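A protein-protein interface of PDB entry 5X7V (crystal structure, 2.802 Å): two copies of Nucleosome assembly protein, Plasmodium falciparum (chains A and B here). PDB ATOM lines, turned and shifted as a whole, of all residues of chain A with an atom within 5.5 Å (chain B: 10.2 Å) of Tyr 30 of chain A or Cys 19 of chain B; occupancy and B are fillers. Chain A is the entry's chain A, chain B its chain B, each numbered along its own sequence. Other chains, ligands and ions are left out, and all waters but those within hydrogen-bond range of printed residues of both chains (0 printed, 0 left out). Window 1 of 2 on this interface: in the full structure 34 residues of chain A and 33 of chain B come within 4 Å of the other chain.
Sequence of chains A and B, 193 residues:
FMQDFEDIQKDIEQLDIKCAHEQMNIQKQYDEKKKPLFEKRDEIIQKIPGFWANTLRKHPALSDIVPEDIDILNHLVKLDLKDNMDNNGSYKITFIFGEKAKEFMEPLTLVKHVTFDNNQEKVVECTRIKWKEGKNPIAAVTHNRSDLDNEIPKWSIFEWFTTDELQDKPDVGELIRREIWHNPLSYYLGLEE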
ATOM      1  N   ILE A  26      -8.898   4.519  22.946  1.00  0.00           N
ATOM      2  CA  ILE A  26      -7.752   5.255  23.479  1.00  0.00           C
ATOM      3  C   ILE A  26      -6.730   5.501  22.372  1.00  0.00           C
ATOM      4  O   ILE A  26      -6.209   6.612  22.247  1.00  0.00           O
ATOM      5  CB  ILE A  26      -7.064   4.546  24.701  1.00  0.00           C
ATOM      6  CG1 ILE A  26      -8.061   4.299  25.844  1.00  0.00           C
ATOM      7  CG2 ILE A  26      -5.896   5.365  25.219  1.00  0.00           C
ATOM      8  CD1 ILE A  26      -8.736   5.529  26.414  1.00  0.00           C
ATOM      9  N   GLN A  27      -6.471   4.495  21.540  1.00  0.00           N
ATOM     10  CA  GLN A  27      -5.488   4.673  20.463  1.00  0.00           C
ATOM     11  C   GLN A  27      -5.775   5.919  19.641  1.00  0.00           C
ATOM     12  O   GLN A  27      -4.850   6.642  19.263  1.00  0.00           O
ATOM     13  CB  GLN A  27      -5.443   3.471  19.522  1.00  0.00           C
ATOM     14  CG  GLN A  27      -4.274   3.536  18.543  1.00  0.00           C
ATOM     15  CD  GLN A  27      -2.975   2.990  19.162  1.00  0.00           C
ATOM     16  OE1 GLN A  27      -2.798   1.775  19.309  1.00  0.00           O
ATOM     17  NE2 GLN A  27      -2.075   3.894  19.550  1.00  0.00           N
ATOM     18  N   LYS A  28      -7.058   6.176  19.382  1.00  0.00           N
ATOM     19  CA  LYS A  28      -7.425   7.228  18.446  1.00  0.00           C
ATOM     20  C   LYS A  28      -7.660   8.521  19.184  1.00  0.00           C
ATOM     21  O   LYS A  28      -7.882   9.554  18.578  1.00  0.00           O
ATOM     22  CB  LYS A  28      -8.652   6.845  17.618  1.00  0.00           C
ATOM     23  CG  LYS A  28      -9.995   6.892  18.334  1.00  0.00           C
ATOM     24  CD  LYS A  28     -11.043   6.014  17.626  1.00  0.00           C
ATOM     25  CE  LYS A  28     -10.789   5.923  16.124  1.00  0.00           C
ATOM     26  NZ  LYS A  28     -11.708   4.957  15.471  1.00  0.00           N
ATOM     27  N   GLN A  29      -7.602   8.462  20.502  1.00  0.00           N
ATOM     28  CA  GLN A  29      -7.499   9.669  21.296  1.00  0.00           C
ATOM     29  C   GLN A  29      -6.139  10.319  21.018  1.00  0.00           C
ATOM     30  O   GLN A  29      -6.057  11.499  20.654  1.00  0.00           O
ATOM     31  CB  GLN A  29      -7.644   9.357  22.786  1.00  0.00           C
ATOM     32  CG  GLN A  29      -9.050   9.100  23.268  1.00  0.00           C
ATOM     33  CD  GLN A  29      -9.170   9.225  24.788  1.00  0.00           C
ATOM     34  OE1 GLN A  29      -8.208   9.553  25.486  1.00  0.00           O
ATOM     35  NE2 GLN A  29     -10.362   8.968  25.304  1.00  0.00           N
ATOM     36  N   TYR A  30      -5.077   9.534  21.173  1.00  0.00           N
ATOM     37  CA  TYR A  30      -3.728  10.069  21.104  1.00  0.00           C
ATOM     38  C   TYR A  30      -3.233  10.307  19.680  1.00  0.00           C
ATOM     39  O   TYR A  30      -2.487  11.253  19.445  1.00  0.00           O
ATOM     40  CB  TYR A  30      -2.773   9.163  21.877  1.00  0.00           C
ATOM     41  CG  TYR A  30      -2.983   9.257  23.372  1.00  0.00           C
ATOM     42  CD1 TYR A  30      -2.256  10.159  24.137  1.00  0.00           C
ATOM     43  CD2 TYR A  30      -3.916   8.462  24.015  1.00  0.00           C
ATOM     44  CE1 TYR A  30      -2.450  10.261  25.498  1.00  0.00           C
ATOM     45  CE2 TYR A  30      -4.114   8.557  25.374  1.00  0.00           C
ATOM     46  CZ  TYR A  30      -3.379   9.459  26.109  1.00  0.00           C
ATOM     47  OH  TYR A  30      -3.565   9.566  27.467  1.00  0.00           O
ATOM     48  N   ASP A  31      -3.661   9.475  18.734  1.00  0.00           N
ATOM     49  CA  ASP A  31      -3.421   9.732  17.307  1.00  0.00           C
ATOM     50  C   ASP A  31      -3.743  11.180  16.955  1.00  0.00           C
ATOM     51  O   ASP A  31      -3.014  11.829  16.203  1.00  0.00           O
ATOM     52  CB  ASP A  31      -4.257   8.792  16.434  1.00  0.00           C
ATOM     53  CG  ASP A  31      -3.593   7.450  16.224  1.00  0.00           C
ATOM     54  OD1 ASP A  31      -2.372   7.348  16.476  1.00  0.00           O
ATOM     55  OD2 ASP A  31      -4.285   6.500  15.804  1.00  0.00           O
ATOM     56  N   GLU A  32      -4.844  11.664  17.521  1.00  0.00           N
ATOM     57  CA  GLU A  32      -5.305  13.033  17.339  1.00  0.00           C
ATOM     58  C   GLU A  32      -4.454  14.033  18.117  1.00  0.00           C
ATOM     59  O   GLU A  32      -4.282  15.177  17.701  1.00  0.00           O
ATOM     60  CB  GLU A  32      -6.766  13.158  17.767  1.00  0.00           C
ATOM     61  CG  GLU A  32      -7.691  13.502  16.616  1.00  0.00           C
ATOM     62  CD  GLU A  32      -9.167  13.549  17.023  1.00  0.00           C
ATOM     63  OE1 GLU A  32      -9.730  14.671  17.058  1.00  0.00           O
ATOM     64  OE2 GLU A  32      -9.766  12.474  17.304  1.00  0.00           O
ATOM     65  N   LYS A  33      -3.922  13.611  19.254  1.00  0.00           N
ATOM     66  CA  LYS A  33      -3.130  14.531  20.042  1.00  0.00           C
ATOM     67  C   LYS A  33      -1.776  14.712  19.370  1.00  0.00           C
ATOM     68  O   LYS A  33      -1.184  15.785  19.397  1.00  0.00           O
ATOM     69  CB  LYS A  33      -3.009  14.037  21.482  1.00  0.00           C
ATOM     70  CG  LYS A  33      -3.953  14.795  22.411  1.00  0.00           C
ATOM     71  CD  LYS A  33      -4.016  14.242  23.817  1.00  0.00           C
ATOM     72  CE  LYS A  33      -5.452  13.938  24.214  1.00  0.00           C
ATOM     73  NZ  LYS A  33      -5.517  13.245  25.538  1.00  0.00           N
ATOM     74  N   LYS A  34      -1.316  13.656  18.725  1.00  0.00           N
ATOM     75  CA  LYS A  34      -0.058  13.674  18.010  1.00  0.00           C
ATOM     76  C   LYS A  34      -0.060  14.601  16.810  1.00  0.00           C
ATOM     77  O   LYS A  34       0.971  15.213  16.523  1.00  0.00           O
ATOM     78  CB  LYS A  34       0.298  12.262  17.552  1.00  0.00           C
ATOM     79  CG  LYS A  34       0.918  11.444  18.642  1.00  0.00           C
ATOM     80  CD  LYS A  34       1.141  10.044  18.194  1.00  0.00           C
ATOM     81  CE  LYS A  34       1.445   9.195  19.385  1.00  0.00           C
ATOM     82  NZ  LYS A  34       1.518   7.782  18.963  1.00  0.00           N
ATOM     83  N   LYS A  35      -1.195  14.689  16.109  1.00  0.00           N
ATOM     84  CA  LYS A  35      -1.282  15.479  14.877  1.00  0.00           C
ATOM     85  C   LYS A  35      -0.553  16.825  14.986  1.00  0.00           C
ATOM     86  O   LYS A  35       0.279  17.122  14.135  1.00  0.00           O
ATOM     87  CB  LYS A  35      -2.744  15.689  14.450  1.00  0.00           C
ATOM     88  CG  LYS A  35      -3.408  14.445  13.935  1.00  0.00           C
ATOM     89  CD  LYS A  35      -4.870  14.690  13.577  1.00  0.00           C
ATOM     90  CE  LYS A  35      -5.024  15.479  12.298  1.00  0.00           C
ATOM     91  NZ  LYS A  35      -4.595  14.635  11.153  1.00  0.00           N
ATOM     92  N   ASP B  11       8.099  14.822  23.387  1.00  0.00           N
ATOM     93  CA  ASP B  11       6.673  15.138  23.362  1.00  0.00           C
ATOM     94  C   ASP B  11       5.843  14.046  22.718  1.00  0.00           C
ATOM     95  O   ASP B  11       4.736  13.735  23.179  1.00  0.00           O
ATOM     96  CB  ASP B  11       6.412  16.428  22.603  1.00  0.00           C
ATOM     97  CG  ASP B  11       6.822  17.660  23.369  1.00  0.00           C
ATOM     98  OD1 ASP B  11       7.537  17.544  24.392  1.00  0.00           O
ATOM     99  OD2 ASP B  11       6.412  18.761  22.932  1.00  0.00           O
ATOM    100  N   ILE B  12       6.354  13.507  21.616  1.00  0.00           N
ATOM    101  CA  ILE B  12       5.682  12.431  20.918  1.00  0.00           C
ATOM    102  C   ILE B  12       5.855  11.156  21.711  1.00  0.00           C
ATOM    103  O   ILE B  12       4.889  10.427  21.934  1.00  0.00           O
ATOM    104  CB  ILE B  12       6.229  12.225  19.491  1.00  0.00           C
ATOM    105  CG1 ILE B  12       5.878  13.410  18.599  1.00  0.00           C
ATOM    106  CG2 ILE B  12       5.688  10.941  18.887  1.00  0.00           C
ATOM    107  CD1 ILE B  12       6.614  13.394  17.295  1.00  0.00           C
ATOM    108  N   GLU B  13       7.086  10.896  22.151  1.00  0.00           N
ATOM    109  CA  GLU B  13       7.371   9.646  22.847  1.00  0.00           C
ATOM    110  C   GLU B  13       6.539   9.505  24.111  1.00  0.00           C
ATOM    111  O   GLU B  13       6.056   8.416  24.412  1.00  0.00           O
ATOM    112  CB  GLU B  13       8.844   9.521  23.216  1.00  0.00           C
ATOM    113  CG  GLU B  13       9.223   8.113  23.677  1.00  0.00           C
ATOM    114  CD  GLU B  13      10.373   8.084  24.700  1.00  0.00           C
ATOM    115  OE1 GLU B  13      10.613   9.118  25.372  1.00  0.00           O
ATOM    116  OE2 GLU B  13      11.030   7.019  24.834  1.00  0.00           O
ATOM    117  N   GLN B  14       6.366  10.583  24.864  1.00  0.00           N
ATOM    118  CA  GLN B  14       5.682  10.422  26.129  1.00  0.00           C
ATOM    119  C   GLN B  14       4.184  10.424  25.955  1.00  0.00           C
ATOM    120  O   GLN B  14       3.459   9.881  26.776  1.00  0.00           O
ATOM    121  CB  GLN B  14       6.125  11.476  27.128  1.00  0.00           C
ATOM    122  CG  GLN B  14       6.957  10.815  28.227  1.00  0.00           C
ATOM    123  CD  GLN B  14       7.485  11.782  29.237  1.00  0.00           C
ATOM    124  OE1 GLN B  14       7.467  12.994  29.018  1.00  0.00           O
ATOM    125  NE2 GLN B  14       7.969  11.258  30.361  1.00  0.00           N
ATOM    126  N   LEU B  15       3.713  10.992  24.864  1.00  0.00           N
ATOM    127  CA  LEU B  15       2.341  10.758  24.455  1.00  0.00           C
ATOM    128  C   LEU B  15       2.194   9.265  24.070  1.00  0.00           C
ATOM    129  O   LEU B  15       1.110   8.678  24.161  1.00  0.00           O
ATOM    130  CB  LEU B  15       1.977  11.681  23.293  1.00  0.00           C
ATOM    131  CG  LEU B  15       0.607  12.346  23.355  1.00  0.00           C
ATOM    132  CD1 LEU B  15       0.368  12.902  24.744  1.00  0.00           C
ATOM    133  CD2 LEU B  15       0.464  13.440  22.289  1.00  0.00           C
ATOM    134  N   ASP B  16       3.292   8.644  23.651  1.00  0.00           N
ATOM    135  CA  ASP B  16       3.238   7.251  23.219  1.00  0.00           C
ATOM    136  C   ASP B  16       3.169   6.388  24.427  1.00  0.00           C
ATOM    137  O   ASP B  16       2.307   5.522  24.541  1.00  0.00           O
ATOM    138  CB  ASP B  16       4.463   6.860  22.392  1.00  0.00           C
ATOM    139  CG  ASP B  16       4.226   6.957  20.906  1.00  0.00           C
ATOM    140  OD1 ASP B  16       3.058   6.977  20.490  1.00  0.00           O
ATOM    141  OD2 ASP B  16       5.217   7.018  20.156  1.00  0.00           O
ATOM    142  N   ILE B  17       4.138   6.606  25.304  1.00  0.00           N
ATOM    143  CA  ILE B  17       4.173   6.013  26.634  1.00  0.00           C
ATOM    144  C   ILE B  17       2.791   6.089  27.302  1.00  0.00           C
ATOM    145  O   ILE B  17       2.219   5.065  27.710  1.00  0.00           O
ATOM    146  CB  ILE B  17       5.229   6.728  27.512  1.00  0.00           C
ATOM    147  CG1 ILE B  17       6.641   6.347  27.060  1.00  0.00           C
ATOM    148  CG2 ILE B  17       5.026   6.398  28.970  1.00  0.00           C
ATOM    149  CD1 ILE B  17       6.814   4.849  26.808  1.00  0.00           C
ATOM    150  N   LYS B  18       2.253   7.278  27.436  1.00  0.00           N
ATOM    151  CA  LYS B  18       0.976   7.359  28.059  1.00  0.00           C
ATOM    152  C   LYS B  18       0.081   6.400  27.368  1.00  0.00           C
ATOM    153  O   LYS B  18      -0.356   5.400  27.905  1.00  0.00           O
ATOM    154  CB  LYS B  18       0.396   8.729  27.878  1.00  0.00           C
ATOM    155  CG  LYS B  18       0.203   9.479  29.168  1.00  0.00           C
ATOM    156  CD  LYS B  18      -0.188  10.909  28.891  1.00  0.00           C
ATOM    157  CE  LYS B  18       0.940  11.851  29.245  1.00  0.00           C
ATOM    158  NZ  LYS B  18       0.489  13.272  29.283  1.00  0.00           N
ATOM    159  N   CYS B  19      -0.128   6.657  26.110  1.00  0.00           N
ATOM    160  CA  CYS B  19      -1.121   5.863  25.427  1.00  0.00           C
ATOM    161  C   CYS B  19      -0.940   4.396  25.811  1.00  0.00           C
ATOM    162  O   CYS B  19      -1.893   3.738  26.221  1.00  0.00           O
ATOM    163  CB  CYS B  19      -1.018   6.063  23.915  1.00  0.00           C
ATOM    164  SG  CYS B  19      -2.147   5.053  22.934  1.00  0.00           S
ATOM    165  N   ALA B  20       0.293   3.899  25.724  1.00  0.00           N
ATOM    166  CA  ALA B  20       0.547   2.495  25.983  1.00  0.00           C
ATOM    167  C   ALA B  20       0.140   2.130  27.399  1.00  0.00           C
ATOM    168  O   ALA B  20      -0.301   1.015  27.673  1.00  0.00           O
ATOM    169  CB  ALA B  20       1.994   2.175  25.750  1.00  0.00           C
ATOM    170  N   HIS B  21       0.285   3.082  28.305  1.00  0.00           N
ATOM    171  CA  HIS B  21      -0.038   2.825  29.686  1.00  0.00           C
ATOM    172  C   HIS B  21      -1.545   2.611  29.848  1.00  0.00           C
ATOM    173  O   HIS B  21      -1.966   1.609  30.396  1.00  0.00           O
ATOM    174  CB  HIS B  21       0.465   3.966  30.557  1.00  0.00           C
ATOM    175  CG  HIS B  21       0.152   3.791  32.008  1.00  0.00           C
ATOM    176  ND1 HIS B  21      -0.772   4.578  32.669  1.00  0.00           N
ATOM    177  CD2 HIS B  21       0.617   2.908  32.921  1.00  0.00           C
ATOM    178  CE1 HIS B  21      -0.857   4.189  33.924  1.00  0.00           C
ATOM    179  NE2 HIS B  21      -0.027   3.175  34.105  1.00  0.00           N
ATOM    180  N   GLU B  22      -2.329   3.547  29.365  1.00  0.00           N
ATOM    181  CA  GLU B  22      -3.744   3.411  29.516  1.00  0.00           C
ATOM    182  C   GLU B  22      -4.253   2.179  28.839  1.00  0.00           C
ATOM    183  O   GLU B  22      -5.178   1.569  29.302  1.00  0.00           O
ATOM    184  CB  GLU B  22      -4.434   4.628  28.958  1.00  0.00           C
ATOM    185  CG  GLU B  22      -3.870   5.914  29.496  1.00  0.00           C
ATOM    186  CD  GLU B  22      -4.729   7.097  29.161  1.00  0.00           C
ATOM    187  OE1 GLU B  22      -5.889   6.892  28.783  1.00  0.00           O
ATOM    188  OE2 GLU B  22      -4.253   8.237  29.284  1.00  0.00           O
ATOM    189  N   GLN B  23      -3.638   1.807  27.735  1.00  0.00           N
ATOM    190  CA  GLN B  23      -4.069   0.654  26.955  1.00  0.00           C
ATOM    191  C   GLN B  23      -3.754  -0.637  27.625  1.00  0.00           C
ATOM    192  O   GLN B  23      -4.407  -1.624  27.420  1.00  0.00           O
ATOM    193  CB  GLN B  23      -3.388   0.664  25.597  1.00  0.00           C
ATOM    194  CG  GLN B  23      -3.919   1.703  24.635  1.00  0.00           C
ATOM    195  CD  GLN B  23      -3.935   1.206  23.219  1.00  0.00           C
ATOM    196  OE1 GLN B  23      -3.034   0.510  22.800  1.00  0.00           O
ATOM    197  NE2 GLN B  23      -4.973   1.547  22.483  1.00  0.00           N
ATOM    198  N   MET B  24      -2.690  -0.629  28.383  1.00  0.00           N
ATOM    199  CA  MET B  24      -2.268  -1.780  29.105  1.00  0.00           C
ATOM    200  C   MET B  24      -3.324  -2.004  30.154  1.00  0.00           C
ATOM    201  O   MET B  24      -3.976  -3.043  30.174  1.00  0.00           O
ATOM    202  CB  MET B  24      -0.972  -1.421  29.770  1.00  0.00           C
ATOM    203  CG  MET B  24      -0.560  -2.385  30.823  1.00  0.00           C
ATOM    204  SD  MET B  24       0.526  -3.508  29.973  1.00  0.00           S
ATOM    205  CE  MET B  24       1.793  -3.760  31.211  1.00  0.00           C
ATOM    206  N   ASN B  25      -3.485  -0.981  30.999  1.00  0.00           N
ATOM    207  CA  ASN B  25      -4.443  -0.919  32.103  1.00  0.00           C
ATOM    208  C   ASN B  25      -5.773  -1.513  31.736  1.00  0.00           C
ATOM    209  O   ASN B  25      -6.476  -2.028  32.555  1.00  0.00           O
ATOM    210  CB  ASN B  25      -4.624   0.516  32.567  1.00  0.00           C
ATOM    211  CG  ASN B  25      -3.580   0.941  33.578  1.00  0.00           C
ATOM    212  OD1 ASN B  25      -3.698   1.989  34.192  1.00  0.00           O
ATOM    213  ND2 ASN B  25      -2.563   0.127  33.760  1.00  0.00           N
ATOM    214  N   ILE B  26      -6.126  -1.383  30.485  1.00  0.00           N
ATOM    215  CA  ILE B  26      -7.298  -1.999  29.932  1.00  0.00           C
ATOM    216  C   ILE B  26      -6.997  -3.472  29.642  1.00  0.00           C
ATOM    217  O   ILE B  26      -7.796  -4.346  29.989  1.00  0.00           O
ATOM    218  CB  ILE B  26      -7.783  -1.249  28.694  1.00  0.00           C
ATOM    219  CG1 ILE B  26      -8.254   0.137  29.127  1.00  0.00           C
ATOM    220  CG2 ILE B  26      -8.914  -1.975  28.033  1.00  0.00           C
ATOM    221  CD1 ILE B  26      -8.523   1.106  28.004  1.00  0.00           C
ATOM    222  N   GLN B  27      -5.834  -3.759  29.071  1.00  0.00           N
ATOM    223  CA  GLN B  27      -5.423  -5.144  28.860  1.00  0.00           C
ATOM    224  C   GLN B  27      -5.628  -5.949  30.150  1.00  0.00           C
ATOM    225  O   GLN B  27      -6.361  -6.934  30.159  1.00  0.00           O
ATOM    226  CB  GLN B  27      -3.964  -5.205  28.398  1.00  0.00           C
ATOM    227  CG  GLN B  27      -3.521  -6.541  27.890  1.00  0.00           C
ATOM    228  CD  GLN B  27      -4.137  -6.872  26.563  1.00  0.00           C
ATOM    229  OE1 GLN B  27      -3.832  -6.244  25.550  1.00  0.00           O
ATOM    230  NE2 GLN B  27      -5.020  -7.863  26.554  1.00  0.00           N
ATOM    231  N   ASN B  87       5.434  -2.082  29.307  1.00  0.00           N
ATOM    232  CA  ASN B  87       5.015  -1.204  28.226  1.00  0.00           C
ATOM    233  C   ASN B  87       5.759  -1.506  26.950  1.00  0.00           C
ATOM    234  O   ASN B  87       5.456  -0.944  25.907  1.00  0.00           O
ATOM    235  CB  ASN B  87       5.205   0.269  28.612  1.00  0.00           C
ATOM    236  CG  ASN B  87       4.126   0.767  29.559  1.00  0.00           C
ATOM    237  OD1 ASN B  87       2.996   0.280  29.531  1.00  0.00           O
ATOM    238  ND2 ASN B  87       4.475   1.735  30.413  1.00  0.00           N
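The side-chain amide nitrogen (NE2) of Gln 27 of chain A sits at hydrogen-bond distance from the side-chain sulfur (SG) of Cys 19 of chain B.
N of Gln 27 of chain A sits close to NE2 of Gln 23 of chain B.
The side-chain amino group (NZ) of Lys 34 of chain A lies within salt-bridge range of the side-chain carboxylate (OD2) of Asp 16 of chain B (3.96 Å).
OH of Tyr 30 of chain A lies close to OE2 of Glu 22 of chain B, at 2.4 Å.
Glu 22 of chain B touches Ile 26 of chain A (OE1 to CG2, 3.9 Å).
Ile 26 of chain A touches Ile 26 of chain B (CG1 to CD1, 3.9 Å).
Leu 15 of chain B touches Tyr 30 of chain A (O to CD1, 3.7 Å).
Lys 18 of chain B touches Tyr 30 of chain A (CD to OH, 3.9 Å).
Cys 19 of chain B touches Tyr 30 of chain A (CB to CD2, 3.8 Å).
Lys 33 of chain A touches Leu 15 of chain B (CB to CD2, 3.6 Å).
CD2 of Leu 15 of chain B touches N of Lys 34 of chain A, at 3.99 Å.
Printed residues of chain B within 4 Å of Ile 26 of chain A: Glu 22 (3.9 Å) and Ile 26 (3.9 Å).
Gln 27 of chain A touches just these residues of chain B: Cys 19 and Gln 23.
Of chain B, only Leu 15 (3.7 Å), Lys 18 (3.9 Å), Cys 19 (3.8 Å) and Glu 22 (2.4 Å) come within 4 Å of Tyr 30 of chain A.
No residue of chain B comes within 4 Å of Asp 31 of chain A.
Of chain B, only Leu 15 (3.6 Å) comes within 4 Å of Lys 33 of chain A.
Printed residues of chain B within 4 Å of Lys 34 of chain A: Leu 15 and Asp 16.
Ile 12 of chain B touches none of the printed residues of chain A.
Of the printed residues of chain A, Asp 16 of chain B touches Lys 34 (2.3 Å).
Printed residues of chain A within 4 Å of Cys 19 of chain B: Gln 27 (3.6 Å) and Tyr 30 (3.8 Å).
Of the printed residues of chain A, Glu 22 of chain B touches Ile 26 and Tyr 30.
Of the printed residues of chain A, Ile 26 of chain B touches Ile 26 (3.9 Å).
The nearest residue of chain A that does not touch Cys 19 of chain B is Ile 26 of chain A (4.4 Å).
Hydrophobic or aromatic side chains of chain A within 4 Å of the printed part of chain B: Ile 26 and Tyr 30.
Among the printed residues, Asp or Glu carboxylates within 4 Å of a Lys or Arg side-chain nitrogen of the other chain: Lys 34 of chain A with Asp 16 of chain B (2.3 Å).
Ile 26 of chain B touches its own counterpart, Ile 26 of chain A.
Of the 11 pairs that touch across the chains among the printed residues, 1 has its exchanged pair printed and touching as well.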
